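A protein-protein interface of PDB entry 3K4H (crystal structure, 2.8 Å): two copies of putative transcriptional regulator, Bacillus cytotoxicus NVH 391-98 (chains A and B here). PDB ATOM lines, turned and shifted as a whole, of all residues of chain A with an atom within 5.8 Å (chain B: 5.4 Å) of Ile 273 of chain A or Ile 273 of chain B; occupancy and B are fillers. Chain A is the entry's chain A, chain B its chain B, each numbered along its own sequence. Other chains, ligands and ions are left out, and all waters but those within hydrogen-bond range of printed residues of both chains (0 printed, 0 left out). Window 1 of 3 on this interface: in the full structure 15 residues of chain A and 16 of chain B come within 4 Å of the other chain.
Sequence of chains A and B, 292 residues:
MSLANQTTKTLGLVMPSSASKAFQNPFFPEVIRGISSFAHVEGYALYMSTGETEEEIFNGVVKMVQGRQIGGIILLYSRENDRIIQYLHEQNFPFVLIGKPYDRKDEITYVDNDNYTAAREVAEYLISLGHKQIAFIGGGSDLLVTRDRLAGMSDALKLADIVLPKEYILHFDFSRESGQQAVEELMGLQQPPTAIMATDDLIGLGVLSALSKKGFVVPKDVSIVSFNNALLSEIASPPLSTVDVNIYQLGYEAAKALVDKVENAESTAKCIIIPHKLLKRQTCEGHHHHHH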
ATOM      1  N   TYR A 110     -23.865 -28.785   5.053  1.00  0.00           N
ATOM      2  CA  TYR A 110     -25.114 -29.455   5.072  1.00  0.00           C
ATOM      3  C   TYR A 110     -26.234 -28.701   4.427  1.00  0.00           C
ATOM      4  O   TYR A 110     -26.146 -27.545   4.277  1.00  0.00           O
ATOM      5  CB  TYR A 110     -25.430 -29.857   6.486  1.00  0.00           C
ATOM      6  CG  TYR A 110     -25.847 -28.759   7.368  1.00  0.00           C
ATOM      7  CD1 TYR A 110     -27.126 -28.333   7.376  1.00  0.00           C
ATOM      8  CD2 TYR A 110     -24.974 -28.178   8.231  1.00  0.00           C
ATOM      9  CE1 TYR A 110     -27.516 -27.362   8.175  1.00  0.00           C
ATOM     10  CE2 TYR A 110     -25.360 -27.192   9.037  1.00  0.00           C
ATOM     11  CZ  TYR A 110     -26.636 -26.784   9.006  1.00  0.00           C
ATOM     12  OH  TYR A 110     -27.050 -25.784   9.824  1.00  0.00           O
ATOM     13  N   VAL A 111     -27.264 -29.409   4.003  1.00  0.00           N
ATOM     14  CA  VAL A 111     -28.458 -28.858   3.402  1.00  0.00           C
ATOM     15  C   VAL A 111     -29.646 -29.194   4.267  1.00  0.00           C
ATOM     16  O   VAL A 111     -29.725 -30.254   4.761  1.00  0.00           O
ATOM     17  CB  VAL A 111     -28.680 -29.437   2.070  1.00  0.00           C
ATOM     18  CG1 VAL A 111     -29.763 -28.775   1.441  1.00  0.00           C
ATOM     19  CG2 VAL A 111     -27.518 -29.257   1.279  1.00  0.00           C
ATOM     20  N   ASP A 112     -30.517 -28.254   4.543  1.00  0.00           N
ATOM     21  CA  ASP A 112     -31.597 -28.516   5.456  1.00  0.00           C
ATOM     22  C   ASP A 112     -32.719 -27.581   5.242  1.00  0.00           C
ATOM     23  O   ASP A 112     -32.594 -26.701   4.501  1.00  0.00           O
ATOM     24  CB  ASP A 112     -31.093 -28.398   6.862  1.00  0.00           C
ATOM     25  CG  ASP A 112     -31.971 -29.039   7.846  1.00  0.00           C
ATOM     26  OD1 ASP A 112     -32.791 -29.841   7.469  1.00  0.00           O
ATOM     27  OD2 ASP A 112     -31.837 -28.747   9.013  1.00  0.00           O
ATOM     28  N   ASN A 113     -33.858 -27.835   5.834  1.00  0.00           N
ATOM     29  CA  ASN A 113     -34.892 -26.847   5.923  1.00  0.00           C
ATOM     30  C   ASN A 113     -34.833 -26.238   7.289  1.00  0.00           C
ATOM     31  O   ASN A 113     -34.291 -26.809   8.156  1.00  0.00           O
ATOM     32  CB  ASN A 113     -36.253 -27.446   5.818  1.00  0.00           C
ATOM     33  CG  ASN A 113     -36.377 -28.401   4.754  1.00  0.00           C
ATOM     34  OD1 ASN A 113     -36.273 -29.562   4.967  1.00  0.00           O
ATOM     35  ND2 ASN A 113     -36.705 -27.939   3.613  1.00  0.00           N
ATOM     36  N   ASP A 114     -35.398 -25.078   7.497  1.00  0.00           N
ATOM     37  CA  ASP A 114     -35.399 -24.520   8.840  1.00  0.00           C
ATOM     38  C   ASP A 114     -36.513 -25.177   9.629  1.00  0.00           C
ATOM     39  O   ASP A 114     -37.574 -24.569   9.883  1.00  0.00           O
ATOM     40  CB  ASP A 114     -35.583 -23.010   8.810  1.00  0.00           C
ATOM     41  CG  ASP A 114     -35.486 -22.386  10.182  1.00  0.00           C
ATOM     42  OD1 ASP A 114     -35.634 -21.162  10.270  1.00  0.00           O
ATOM     43  OD2 ASP A 114     -35.279 -23.115  11.176  1.00  0.00           O
ATOM     44  N   LYS A 270     -20.403 -24.360   4.627  1.00  0.00           N
ATOM     45  CA  LYS A 270     -21.601 -23.545   4.718  1.00  0.00           C
ATOM     46  C   LYS A 270     -22.793 -24.444   4.996  1.00  0.00           C
ATOM     47  O   LYS A 270     -22.695 -25.662   4.912  1.00  0.00           O
ATOM     48  CB  LYS A 270     -21.835 -22.831   3.389  1.00  0.00           C
ATOM     49  CG  LYS A 270     -21.757 -23.779   2.202  1.00  0.00           C
ATOM     50  CD  LYS A 270     -21.875 -23.055   0.895  1.00  0.00           C
ATOM     51  CE  LYS A 270     -20.730 -23.457  -0.028  1.00  0.00           C
ATOM     52  NZ  LYS A 270     -21.240 -24.030  -1.324  1.00  0.00           N
ATOM     53  N   CYS A 271     -23.922 -23.818   5.289  1.00  0.00           N
ATOM     54  CA  CYS A 271     -25.196 -24.476   5.419  1.00  0.00           C
ATOM     55  C   CYS A 271     -26.157 -23.894   4.381  1.00  0.00           C
ATOM     56  O   CYS A 271     -26.162 -22.699   4.160  1.00  0.00           O
ATOM     57  CB  CYS A 271     -25.686 -24.229   6.837  1.00  0.00           C
ATOM     58  SG  CYS A 271     -27.446 -24.204   7.070  1.00  0.00           S
ATOM     59  N   ILE A 272     -26.974 -24.721   3.750  1.00  0.00           N
ATOM     60  CA  ILE A 272     -27.924 -24.253   2.727  1.00  0.00           C
ATOM     61  C   ILE A 272     -29.361 -24.515   3.160  1.00  0.00           C
ATOM     62  O   ILE A 272     -29.739 -25.655   3.385  1.00  0.00           O
ATOM     63  CB  ILE A 272     -27.647 -24.915   1.350  1.00  0.00           C
ATOM     64  CG1 ILE A 272     -26.192 -24.630   0.949  1.00  0.00           C
ATOM     65  CG2 ILE A 272     -28.595 -24.398   0.308  1.00  0.00           C
ATOM     66  CD1 ILE A 272     -25.768 -25.030  -0.468  1.00  0.00           C
ATOM     67  N   ILE A 273     -30.168 -23.467   3.285  1.00  0.00           N
ATOM     68  CA  ILE A 273     -31.526 -23.635   3.799  1.00  0.00           C
ATOM     69  C   ILE A 273     -32.553 -23.530   2.677  1.00  0.00           C
ATOM     70  O   ILE A 273     -32.699 -22.461   2.061  1.00  0.00           O
ATOM     71  CB  ILE A 273     -31.847 -22.629   4.928  1.00  0.00           C
ATOM     72  CG1 ILE A 273     -30.859 -22.770   6.086  1.00  0.00           C
ATOM     73  CG2 ILE A 273     -33.279 -22.803   5.436  1.00  0.00           C
ATOM     74  CD1 ILE A 273     -30.702 -24.172   6.649  1.00  0.00           C
ATOM     75  N   ILE A 274     -33.257 -24.631   2.422  1.00  0.00           N
ATOM     76  CA  ILE A 274     -34.252 -24.707   1.355  1.00  0.00           C
ATOM     77  C   ILE A 274     -35.611 -24.336   1.951  1.00  0.00           C
ATOM     78  O   ILE A 274     -35.972 -24.826   3.023  1.00  0.00           O
ATOM     79  CB  ILE A 274     -34.274 -26.154   0.746  1.00  0.00           C
ATOM     80  CG1 ILE A 274     -33.318 -26.308  -0.442  1.00  0.00           C
ATOM     81  CG2 ILE A 274     -35.650 -26.546   0.259  1.00  0.00           C
ATOM     82  CD1 ILE A 274     -31.856 -26.218  -0.111  1.00  0.00           C
ATOM     83  N   PRO A 275     -36.392 -23.487   1.266  1.00  0.00           N
ATOM     84  CA  PRO A 275     -37.672 -23.074   1.824  1.00  0.00           C
ATOM     85  C   PRO A 275     -38.674 -24.199   1.963  1.00  0.00           C
ATOM     86  O   PRO A 275     -38.720 -25.133   1.143  1.00  0.00           O
ATOM     87  CB  PRO A 275     -38.210 -22.093   0.795  1.00  0.00           C
ATOM     88  CG  PRO A 275     -37.039 -21.686  -0.015  1.00  0.00           C
ATOM     89  CD  PRO A 275     -36.196 -22.924  -0.070  1.00  0.00           C
ATOM     90  N   TYR B 110     -30.325 -15.384  -0.811  1.00  0.00           N
ATOM     91  CA  TYR B 110     -29.669 -14.501   0.097  1.00  0.00           C
ATOM     92  C   TYR B 110     -28.763 -15.234   1.045  1.00  0.00           C
ATOM     93  O   TYR B 110     -28.731 -16.458   1.122  1.00  0.00           O
ATOM     94  CB  TYR B 110     -30.702 -13.652   0.844  1.00  0.00           C
ATOM     95  CG  TYR B 110     -31.543 -14.380   1.869  1.00  0.00           C
ATOM     96  CD1 TYR B 110     -31.179 -14.360   3.206  1.00  0.00           C
ATOM     97  CD2 TYR B 110     -32.719 -15.056   1.509  1.00  0.00           C
ATOM     98  CE1 TYR B 110     -31.944 -14.994   4.185  1.00  0.00           C
ATOM     99  CE2 TYR B 110     -33.506 -15.720   2.494  1.00  0.00           C
ATOM    100  CZ  TYR B 110     -33.096 -15.663   3.833  1.00  0.00           C
ATOM    101  OH  TYR B 110     -33.786 -16.273   4.839  1.00  0.00           O
ATOM    102  N   ASP B 112     -27.024 -15.018   5.003  1.00  0.00           N
ATOM    103  CA  ASP B 112     -27.368 -14.504   6.323  1.00  0.00           C
ATOM    104  C   ASP B 112     -26.655 -15.216   7.475  1.00  0.00           C
ATOM    105  O   ASP B 112     -25.993 -16.259   7.302  1.00  0.00           O
ATOM    106  CB  ASP B 112     -28.884 -14.593   6.518  1.00  0.00           C
ATOM    107  CG  ASP B 112     -29.424 -13.586   7.532  1.00  0.00           C
ATOM    108  OD1 ASP B 112     -28.667 -12.702   7.997  1.00  0.00           O
ATOM    109  OD2 ASP B 112     -30.637 -13.686   7.858  1.00  0.00           O
ATOM    110  N   ASN B 113     -26.775 -14.621   8.655  1.00  0.00           N
ATOM    111  CA  ASN B 113     -26.439 -15.291   9.897  1.00  0.00           C
ATOM    112  C   ASN B 113     -27.732 -15.784  10.541  1.00  0.00           C
ATOM    113  O   ASN B 113     -28.803 -15.215  10.314  1.00  0.00           O
ATOM    114  CB  ASN B 113     -25.767 -14.305  10.854  1.00  0.00           C
ATOM    115  CG  ASN B 113     -24.349 -14.010  10.481  1.00  0.00           C
ATOM    116  OD1 ASN B 113     -24.021 -12.877  10.153  1.00  0.00           O
ATOM    117  ND2 ASN B 113     -23.487 -15.030  10.528  1.00  0.00           N
ATOM    118  N   ASP B 114     -27.653 -16.743  11.434  1.00  0.00           N
ATOM    119  CA  ASP B 114     -28.843 -17.109  12.148  1.00  0.00           C
ATOM    120  C   ASP B 114     -28.950 -16.163  13.268  1.00  0.00           C
ATOM    121  O   ASP B 114     -28.645 -16.471  14.359  1.00  0.00           O
ATOM    122  CB  ASP B 114     -28.754 -18.492  12.725  1.00  0.00           C
ATOM    123  CG  ASP B 114     -30.070 -19.003  13.164  1.00  0.00           C
ATOM    124  OD1 ASP B 114     -30.169 -20.195  13.404  1.00  0.00           O
ATOM    125  OD2 ASP B 114     -31.008 -18.223  13.259  1.00  0.00           O
ATOM    126  N   ALA B 269     -33.941 -20.700  -5.370  1.00  0.00           N
ATOM    127  CA  ALA B 269     -33.763 -19.714  -4.379  1.00  0.00           C
ATOM    128  C   ALA B 269     -33.484 -20.442  -3.143  1.00  0.00           C
ATOM    129  O   ALA B 269     -34.222 -21.277  -2.752  1.00  0.00           O
ATOM    130  CB  ALA B 269     -35.004 -19.026  -4.221  1.00  0.00           C
ATOM    131  N   LYS B 270     -32.392 -20.101  -2.512  1.00  0.00           N
ATOM    132  CA  LYS B 270     -32.016 -20.725  -1.304  1.00  0.00           C
ATOM    133  C   LYS B 270     -31.443 -19.676  -0.460  1.00  0.00           C
ATOM    134  O   LYS B 270     -31.042 -18.675  -0.918  1.00  0.00           O
ATOM    135  CB  LYS B 270     -30.938 -21.713  -1.576  1.00  0.00           C
ATOM    136  CG  LYS B 270     -30.325 -21.486  -2.864  1.00  0.00           C
ATOM    137  CD  LYS B 270     -28.898 -21.796  -2.818  1.00  0.00           C
ATOM    138  CE  LYS B 270     -28.361 -21.851  -4.204  1.00  0.00           C
ATOM    139  NZ  LYS B 270     -26.962 -22.311  -4.261  1.00  0.00           N
ATOM    140  N   CYS B 271     -31.445 -19.935   0.812  1.00  0.00           N
ATOM    141  CA  CYS B 271     -30.784 -19.116   1.794  1.00  0.00           C
ATOM    142  C   CYS B 271     -29.475 -19.792   2.170  1.00  0.00           C
ATOM    143  O   CYS B 271     -29.458 -20.985   2.479  1.00  0.00           O
ATOM    144  CB  CYS B 271     -31.656 -18.990   3.020  1.00  0.00           C
ATOM    145  SG  CYS B 271     -30.812 -18.218   4.395  1.00  0.00           S
ATOM    146  N   ILE B 272     -28.376 -19.041   2.136  1.00  0.00           N
ATOM    147  CA  ILE B 272     -27.092 -19.577   2.551  1.00  0.00           C
ATOM    148  C   ILE B 272     -26.801 -18.983   3.904  1.00  0.00           C
ATOM    149  O   ILE B 272     -26.915 -17.776   4.071  1.00  0.00           O
ATOM    150  CB  ILE B 272     -25.985 -19.224   1.532  1.00  0.00           C
ATOM    151  CG1 ILE B 272     -26.491 -19.499   0.115  1.00  0.00           C
ATOM    152  CG2 ILE B 272     -24.726 -20.022   1.812  1.00  0.00           C
ATOM    153  CD1 ILE B 272     -25.807 -18.703  -0.947  1.00  0.00           C
ATOM    154  N   ILE B 273     -26.448 -19.821   4.874  1.00  0.00           N
ATOM    155  CA  ILE B 273     -26.338 -19.382   6.282  1.00  0.00           C
ATOM    156  C   ILE B 273     -24.909 -19.520   6.787  1.00  0.00           C
ATOM    157  O   ILE B 273     -24.321 -20.604   6.761  1.00  0.00           O
ATOM    158  CB  ILE B 273     -27.325 -20.154   7.229  1.00  0.00           C
ATOM    159  CG1 ILE B 273     -28.788 -19.772   6.962  1.00  0.00           C
ATOM    160  CG2 ILE B 273     -27.026 -19.862   8.684  1.00  0.00           C
ATOM    161  CD1 ILE B 273     -29.112 -18.349   7.279  1.00  0.00           C
ATOM    162  N   ILE B 274     -24.364 -18.404   7.246  1.00  0.00           N
ATOM    163  CA  ILE B 274     -22.984 -18.316   7.697  1.00  0.00           C
ATOM    164  C   ILE B 274     -22.948 -18.543   9.207  1.00  0.00           C
ATOM    165  O   ILE B 274     -23.793 -18.003   9.933  1.00  0.00           O
ATOM    166  CB  ILE B 274     -22.363 -16.938   7.248  1.00  0.00           C
ATOM    167  CG1 ILE B 274     -21.590 -17.097   5.945  1.00  0.00           C
ATOM    168  CG2 ILE B 274     -21.406 -16.350   8.284  1.00  0.00           C
ATOM    169  CD1 ILE B 274     -22.414 -17.609   4.800  1.00  0.00           C
ATOM    170  N   PRO B 275     -21.995 -19.370   9.688  1.00  0.00           N
ATOM    171  CA  PRO B 275     -21.957 -19.654  11.117  1.00  0.00           C
ATOM    172  C   PRO B 275     -21.521 -18.451  11.908  1.00  0.00           C
ATOM    173  O   PRO B 275     -20.799 -17.600  11.396  1.00  0.00           O
ATOM    174  CB  PRO B 275     -20.928 -20.764  11.243  1.00  0.00           C
ATOM    175  CG  PRO B 275     -20.196 -20.769   9.993  1.00  0.00           C
ATOM    176  CD  PRO B 275     -21.040 -20.196   8.937  1.00  0.00           C
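Cys 271 of chain A touches Ile 272 of chain B, and with the chains exchanged Ile 272 of chain A touches Cys 271 of chain B.
Cys 271 of chain A touches Ile 273 of chain B, and with the chains exchanged Ile 273 of chain A touches Cys 271 of chain B.
Ile 273 of chain A touches Lys 270 of chain B, but with the chains exchanged Lys 270 of chain A does not touch Ile 273 of chain B (4.5 Å).
Ile 273 of chain B touches its own counterpart, Ile 273 of chain A.
Val 111 of chain A touches none of the printed residues of chain B.
Of the printed residues of chain B, Cys 271 of chain A touches Ile 272 (3.6 Å) and Ile 273 (3.0 Å).
Of the printed residues of chain B, Ile 272 of chain A touches Cys 271 (3.6 Å).
Of the printed residues of chain B, Ile 273 of chain A touches Lys 270 (3.8 Å), Cys 271 (2.7 Å) and Ile 273 (3.7 Å).
Of the printed residues of chain A, Ala 269 of chain B touches Pro 275.
Of the printed residues of chain A, Ile 272 of chain B touches Cys 271 (3.6 Å).
Ile 273 of chain B touches two residues of chain A.
The nearest residue of chain A that does not touch Ile 273 of chain B is Lys 270 of chain A (4.5 Å).
The backbone NH (N) of Tyr 110 of chain B lies within hydrogen-bond range of the backbone carbonyl oxygen (O) of Lys 270 of chain B, 3.4 Å away.
O of Ile 272 of chain A is in hydrogen-bond range of N of Asp 112 of chain A (2.9 Å).
The backbone carbonyl oxygen (O) of Ile 272 of chain B is in hydrogen-bond range of the backbone NH (N) of Asp 112 of chain B (2.9 Å).
OH of Tyr 110 of chain A is in hydrogen-bond range of SG of Cys 271 of chain A (3.2 Å).
The side-chain sulfur (SG) of Cys 271 of chain B lies close to the side-chain hydroxyl (OH) of Tyr 110 of chain B.
O of Tyr 110 of chain A lies within hydrogen-bond range of N of Ile 272 of chain A (3.0 Å).
Among the printed residues, pairs that only touch across the chains: Cys 271 of chain A with Ile 272 of chain B, Ile 272 of chain A with Cys 271 of chain B, Ile 273 of chain A with Lys 270 of chain B, Ile 273 of chain A with Ile 273 of chain B and Pro 275 of chain A with Ala 269 of chain B.
Of the 11 printed residues of chain B, 5 touch a printed residue of chain A.
Hydrophobic or aromatic side chains of chain B within 4 Å of the printed part of chain A: Ile 272 and Ile 273.
Along chain B the printed residues that touch a printed residue of chain A span positions 269 to 273.
Of the 11 printed residues of chain A, 4 touch a printed residue of chain B.
Among the printed residues, no Asp or Glu carboxylate lies within 4 Å of a Lys or Arg side-chain nitrogen of the other chain.
The backbone carbonyl oxygen (O) of Cys 271 of chain A is in hydrogen-bond range of the backbone NH (N) of Ile 273 of chain B, 3.0 Å away.
N of Ile 273 of chain A is in hydrogen-bond range of O of Cys 271 of chain B (2.7 Å).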
